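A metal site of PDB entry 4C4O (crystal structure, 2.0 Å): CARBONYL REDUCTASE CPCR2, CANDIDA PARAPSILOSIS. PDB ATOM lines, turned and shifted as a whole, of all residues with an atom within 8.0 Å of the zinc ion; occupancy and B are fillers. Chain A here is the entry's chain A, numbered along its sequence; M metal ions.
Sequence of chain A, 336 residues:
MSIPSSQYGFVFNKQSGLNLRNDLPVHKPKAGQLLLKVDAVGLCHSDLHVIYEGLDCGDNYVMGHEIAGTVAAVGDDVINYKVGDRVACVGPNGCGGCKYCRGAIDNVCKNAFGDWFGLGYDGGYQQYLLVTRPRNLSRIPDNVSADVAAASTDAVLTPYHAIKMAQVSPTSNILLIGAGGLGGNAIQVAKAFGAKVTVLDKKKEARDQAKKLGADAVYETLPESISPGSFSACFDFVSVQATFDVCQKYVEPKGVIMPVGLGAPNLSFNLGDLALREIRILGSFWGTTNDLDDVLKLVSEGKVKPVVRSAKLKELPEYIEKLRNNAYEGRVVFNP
The side-chain sulfur (SG) of Cys 109 lies close to the backbone NH (N) of Asn 111, at 3.7 Å.
The backbone NH (N) of Ala 112 sits close to the side-chain sulfur (SG) of Cys 109 (3.5 Å).
The backbone NH (N) of Gly 96 lies close to the side-chain sulfur (SG) of Cys 101 (3.3 Å).
SG of Cys 98 sits close to N of Tyr 100, at 3.5 Å.
The side-chain sulfur (SG) of Cys 95 sits close to the backbone NH (N) of Gly 97, at 3.3 Å.
SG of Cys 95 lies close to ND2 of Asn 111 (3.4 Å).
N of Gly 96 touches the zinc ion, at 3.7 Å.
Within 4 Å of the zinc ion: Cys 95, Gly 96, Cys 98, Cys 101 and Cys 109.
The zinc ion is bound by the side-chain sulfur of Cys 109 (2.3 Å), the side-chain sulfur of Cys 101 (2.3 Å), the side-chain sulfur of Cys 98 (2.3 Å) and the side-chain sulfur of Cys 95 (2.4 Å).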
ATOM      1  N   PRO A  92       2.803   5.519 -16.721  1.00  0.00           N
ATOM      2  CA  PRO A  92       3.818   4.451 -16.530  1.00  0.00           C
ATOM      3  C   PRO A  92       4.332   4.347 -15.096  1.00  0.00           C
ATOM      4  O   PRO A  92       4.930   3.351 -14.753  1.00  0.00           O
ATOM      5  CB  PRO A  92       4.941   4.862 -17.485  1.00  0.00           C
ATOM      6  CG  PRO A  92       4.194   5.583 -18.592  1.00  0.00           C
ATOM      7  CD  PRO A  92       3.151   6.388 -17.850  1.00  0.00           C
ATOM      8  N   ASN A  93       4.110   5.395 -14.286  1.00  0.00           N
ATOM      9  CA  ASN A  93       4.348   5.274 -12.861  1.00  0.00           C
ATOM     10  C   ASN A  93       5.744   4.654 -12.507  1.00  0.00           C
ATOM     11  O   ASN A  93       5.838   3.763 -11.693  1.00  0.00           O
ATOM     12  CB  ASN A  93       3.234   4.388 -12.229  1.00  0.00           C
ATOM     13  CG  ASN A  93       3.182   4.524 -10.700  1.00  0.00           C
ATOM     14  OD1 ASN A  93       3.614   5.542 -10.155  1.00  0.00           O
ATOM     15  ND2 ASN A  93       2.640   3.534 -10.009  1.00  0.00           N
ATOM     16  N   GLY A  94       6.823   5.142 -13.137  1.00  0.00           N
ATOM     17  CA  GLY A  94       8.151   4.598 -12.920  1.00  0.00           C
ATOM     18  C   GLY A  94       8.611   4.548 -11.434  1.00  0.00           C
ATOM     19  O   GLY A  94       8.271   5.434 -10.644  1.00  0.00           O
ATOM     20  N   CYS A  95       9.510   3.615 -11.130  1.00  0.00           N
ATOM     21  CA  CYS A  95      10.062   3.454  -9.781  1.00  0.00           C
ATOM     22  C   CYS A  95      10.866   4.659  -9.269  1.00  0.00           C
ATOM     23  O   CYS A  95      10.920   4.907  -8.077  1.00  0.00           O
ATOM     24  CB  CYS A  95      10.915   2.177  -9.697  1.00  0.00           C
ATOM     25  SG  CYS A  95      12.604   2.273 -10.362  1.00  0.00           S
ATOM     26  N   GLY A  96      11.495   5.418 -10.162  1.00  0.00           N
ATOM     27  CA  GLY A  96      12.274   6.582  -9.717  1.00  0.00           C
ATOM     28  C   GLY A  96      13.689   6.271  -9.218  1.00  0.00           C
ATOM     29  O   GLY A  96      14.438   7.173  -8.959  1.00  0.00           O
ATOM     30  N   GLY A  97      14.063   4.992  -9.105  1.00  0.00           N
ATOM     31  CA  GLY A  97      15.354   4.592  -8.547  1.00  0.00           C
ATOM     32  C   GLY A  97      16.280   3.843  -9.504  1.00  0.00           C
ATOM     33  O   GLY A  97      17.447   3.681  -9.195  1.00  0.00           O
ATOM     34  N   CYS A  98      15.815   3.457 -10.688  1.00  0.00           N
ATOM     35  CA  CYS A  98      16.637   2.687 -11.604  1.00  0.00           C
ATOM     36  C   CYS A  98      17.285   3.604 -12.665  1.00  0.00           C
ATOM     37  O   CYS A  98      17.043   4.824 -12.692  1.00  0.00           O
ATOM     38  CB  CYS A  98      15.761   1.629 -12.269  1.00  0.00           C
ATOM     39  SG  CYS A  98      14.676   2.343 -13.542  1.00  0.00           S
ATOM     40  N   LYS A  99      18.139   3.022 -13.512  1.00  0.00           N
ATOM     41  CA  LYS A  99      18.905   3.826 -14.487  1.00  0.00           C
ATOM     42  C   LYS A  99      17.977   4.405 -15.553  1.00  0.00           C
ATOM     43  O   LYS A  99      18.254   5.495 -16.049  1.00  0.00           O
ATOM     44  CB  LYS A  99      20.022   3.010 -15.157  1.00  0.00           C
ATOM     45  CG  LYS A  99      19.557   1.832 -16.016  1.00  0.00           C
ATOM     46  CD  LYS A  99      20.779   1.148 -16.614  1.00  0.00           C
ATOM     47  CE  LYS A  99      20.414   0.041 -17.597  1.00  0.00           C
ATOM     48  NZ  LYS A  99      21.600  -0.380 -18.407  1.00  0.00           N
ATOM     49  N   TYR A 100      16.898   3.695 -15.876  1.00  0.00           N
ATOM     50  CA  TYR A 100      15.934   4.211 -16.846  1.00  0.00           C
ATOM     51  C   TYR A 100      15.260   5.451 -16.286  1.00  0.00           C
ATOM     52  O   TYR A 100      15.234   6.496 -16.953  1.00  0.00           O
ATOM     53  CB  TYR A 100      14.931   3.125 -17.330  1.00  0.00           C
ATOM     54  CG  TYR A 100      15.678   1.945 -17.941  1.00  0.00           C
ATOM     55  CD1 TYR A 100      16.297   2.051 -19.202  1.00  0.00           C
ATOM     56  CD2 TYR A 100      15.836   0.776 -17.230  1.00  0.00           C
ATOM     57  CE1 TYR A 100      16.997   0.982 -19.753  1.00  0.00           C
ATOM     58  CE2 TYR A 100      16.537  -0.300 -17.760  1.00  0.00           C
ATOM     59  CZ  TYR A 100      17.115  -0.189 -19.021  1.00  0.00           C
ATOM     60  OH  TYR A 100      17.801  -1.277 -19.512  1.00  0.00           O
ATOM     61  N   CYS A 101      14.761   5.353 -15.058  1.00  0.00           N
ATOM     62  CA  CYS A 101      14.088   6.500 -14.442  1.00  0.00           C
ATOM     63  C   CYS A 101      15.026   7.703 -14.214  1.00  0.00           C
ATOM     64  O   CYS A 101      14.581   8.863 -14.304  1.00  0.00           O
ATOM     65  CB  CYS A 101      13.400   6.075 -13.135  1.00  0.00           C
ATOM     66  SG  CYS A 101      11.991   4.976 -13.371  1.00  0.00           S
ATOM     67  N   ARG A 102      16.313   7.461 -13.996  1.00  0.00           N
ATOM     68  CA  ARG A 102      17.206   8.543 -13.521  1.00  0.00           C
ATOM     69  C   ARG A 102      17.970   9.493 -14.504  1.00  0.00           C
ATOM     70  O   ARG A 102      18.365  10.562 -14.049  1.00  0.00           O
ATOM     71  CB  ARG A 102      18.211   7.960 -12.513  1.00  0.00           C
ATOM     72  CG  ARG A 102      17.594   7.598 -11.162  1.00  0.00           C
ATOM     73  CD  ARG A 102      18.645   7.221 -10.144  1.00  0.00           C
ATOM     74  NE  ARG A 102      19.726   6.490 -10.791  1.00  0.00           N
ATOM     75  CZ  ARG A 102      20.231   5.341 -10.382  1.00  0.00           C
ATOM     76  NH1 ARG A 102      19.831   4.746  -9.264  1.00  0.00           N
ATOM     77  NH2 ARG A 102      21.192   4.776 -11.117  1.00  0.00           N
ATOM     78  N   ILE A 105      14.000   8.440 -18.850  1.00  0.00           N
ATOM     79  CA  ILE A 105      13.166   7.512 -19.594  1.00  0.00           C
ATOM     80  C   ILE A 105      12.393   6.645 -18.605  1.00  0.00           C
ATOM     81  O   ILE A 105      12.398   5.398 -18.668  1.00  0.00           O
ATOM     82  CB  ILE A 105      13.962   6.703 -20.629  1.00  0.00           C
ATOM     83  CG1 ILE A 105      15.156   6.003 -19.970  1.00  0.00           C
ATOM     84  CG2 ILE A 105      14.461   7.666 -21.724  1.00  0.00           C
ATOM     85  N   ASP A 106      11.617   7.323 -17.762  1.00  0.00           N
ATOM     86  CA  ASP A 106      10.837   6.621 -16.749  1.00  0.00           C
ATOM     87  C   ASP A 106       9.652   5.866 -17.375  1.00  0.00           C
ATOM     88  O   ASP A 106       9.015   5.076 -16.683  1.00  0.00           O
ATOM     89  CB  ASP A 106      10.416   7.523 -15.590  1.00  0.00           C
ATOM     90  CG  ASP A 106       9.654   8.823 -16.023  1.00  0.00           C
ATOM     91  OD1 ASP A 106       9.113   8.924 -17.129  1.00  0.00           O
ATOM     92  OD2 ASP A 106       9.551   9.750 -15.200  1.00  0.00           O
ATOM     93  N   ASN A 107       9.350   6.113 -18.655  1.00  0.00           N
ATOM     94  CA  ASN A 107       8.289   5.344 -19.344  1.00  0.00           C
ATOM     95  C   ASN A 107       8.672   3.871 -19.641  1.00  0.00           C
ATOM     96  O   ASN A 107       7.758   3.075 -19.873  1.00  0.00           O
ATOM     97  CB  ASN A 107       7.828   6.031 -20.612  1.00  0.00           C
ATOM     98  CG  ASN A 107       8.967   6.214 -21.624  1.00  0.00           C
ATOM     99  OD1 ASN A 107      10.121   6.469 -21.252  1.00  0.00           O
ATOM    100  ND2 ASN A 107       8.645   6.075 -22.890  1.00  0.00           N
ATOM    101  N   VAL A 108       9.970   3.507 -19.630  1.00  0.00           N
ATOM    102  CA  VAL A 108      10.389   2.111 -19.882  1.00  0.00           C
ATOM    103  C   VAL A 108      10.973   1.437 -18.630  1.00  0.00           C
ATOM    104  O   VAL A 108      11.764   0.518 -18.748  1.00  0.00           O
ATOM    105  CB  VAL A 108      11.391   1.968 -21.066  1.00  0.00           C
ATOM    106  CG1 VAL A 108      10.771   2.499 -22.355  1.00  0.00           C
ATOM    107  CG2 VAL A 108      12.721   2.679 -20.784  1.00  0.00           C
ATOM    108  N   CYS A 109      10.589   1.920 -17.456  1.00  0.00           N
ATOM    109  CA  CYS A 109      11.033   1.336 -16.188  1.00  0.00           C
ATOM    110  C   CYS A 109      10.647  -0.146 -16.081  1.00  0.00           C
ATOM    111  O   CYS A 109       9.465  -0.468 -16.022  1.00  0.00           O
ATOM    112  CB  CYS A 109      10.384   2.108 -15.046  1.00  0.00           C
ATOM    113  SG  CYS A 109      10.799   1.530 -13.377  1.00  0.00           S
ATOM    114  N   LYS A 110      11.642  -1.012 -15.968  1.00  0.00           N
ATOM    115  CA  LYS A 110      11.380  -2.466 -15.738  1.00  0.00           C
ATOM    116  C   LYS A 110      10.671  -2.742 -14.398  1.00  0.00           C
ATOM    117  O   LYS A 110       9.746  -3.536 -14.320  1.00  0.00           O
ATOM    118  CB  LYS A 110      12.699  -3.293 -15.785  1.00  0.00           C
ATOM    119  CG  LYS A 110      13.471  -3.223 -17.111  1.00  0.00           C
ATOM    120  CD  LYS A 110      14.490  -4.368 -17.226  1.00  0.00           C
ATOM    121  CE  LYS A 110      15.469  -4.157 -18.370  1.00  0.00           C
ATOM    122  NZ  LYS A 110      16.115  -5.418 -18.917  1.00  0.00           N
ATOM    123  N   ASN A 111      11.144  -2.113 -13.333  1.00  0.00           N
ATOM    124  CA  ASN A 111      10.519  -2.307 -12.010  1.00  0.00           C
ATOM    125  C   ASN A 111       9.022  -1.912 -11.907  1.00  0.00           C
ATOM    126  O   ASN A 111       8.339  -2.374 -11.010  1.00  0.00           O
ATOM    127  CB  ASN A 111      11.260  -1.505 -10.957  1.00  0.00           C
ATOM    128  CG  ASN A 111      12.719  -1.909 -10.822  1.00  0.00           C
ATOM    129  OD1 ASN A 111      13.071  -3.048 -11.076  1.00  0.00           O
ATOM    130  ND2 ASN A 111      13.567  -0.957 -10.450  1.00  0.00           N
ATOM    131  N   ALA A 112       8.505  -1.103 -12.841  1.00  0.00           N
ATOM    132  CA  ALA A 112       7.104  -0.652 -12.791  1.00  0.00           C
ATOM    133  C   ALA A 112       6.178  -1.443 -13.737  1.00  0.00           C
ATOM    134  O   ALA A 112       4.975  -1.174 -13.811  1.00  0.00           O
ATOM    135  CB  ALA A 112       7.021   0.810 -13.122  1.00  0.00           C
ATOM    136  N   ARG A 133       3.904   7.063  -5.520  1.00  0.00           N
ATOM    137  CA  ARG A 133       5.114   7.656  -6.097  1.00  0.00           C
ATOM    138  C   ARG A 133       4.780   9.021  -6.701  1.00  0.00           C
ATOM    139  O   ARG A 133       4.599   9.158  -7.909  1.00  0.00           O
ATOM    140  CB  ARG A 133       5.716   6.734  -7.169  1.00  0.00           C
ATOM    141  CG  ARG A 133       6.471   5.490  -6.681  1.00  0.00           C
ATOM    142  CD  ARG A 133       6.947   4.626  -7.898  1.00  0.00           C
ATOM    143  NE  ARG A 133       6.873   3.168  -7.665  1.00  0.00           N
ATOM    144  CZ  ARG A 133       6.315   2.249  -8.459  1.00  0.00           C
ATOM    145  NH1 ARG A 133       5.672   2.525  -9.590  1.00  0.00           N
ATOM    146  NH2 ARG A 133       6.396   0.972  -8.095  1.00  0.00           N
ATOM    147  N   ARG A 135       6.534  11.429  -7.549  1.00  0.00           N
ATOM    148  CA  ARG A 135       7.358  11.887  -8.643  1.00  0.00           C
ATOM    149  C   ARG A 135       6.606  11.775  -9.990  1.00  0.00           C
ATOM    150  O   ARG A 135       6.933  12.487 -10.951  1.00  0.00           O
ATOM    151  CB  ARG A 135       8.663  11.093  -8.726  1.00  0.00           C
ATOM    152  CG  ARG A 135       8.502   9.694  -9.290  1.00  0.00           C
ATOM    153  CD  ARG A 135       9.869   9.015  -9.500  1.00  0.00           C
ATOM    154  NE  ARG A 135      10.746   9.508 -10.586  1.00  0.00           N
ATOM    155  CZ  ARG A 135      10.618   9.339 -11.909  1.00  0.00           C
ATOM    156  NH1 ARG A 135       9.574   8.715 -12.470  1.00  0.00           N
ATOM    157  NH2 ARG A 135      11.573   9.854 -12.678  1.00  0.00           N
HETATM  158 ZN    ZN M   1      12.557   2.825 -12.654  1.00  0.00          ZN
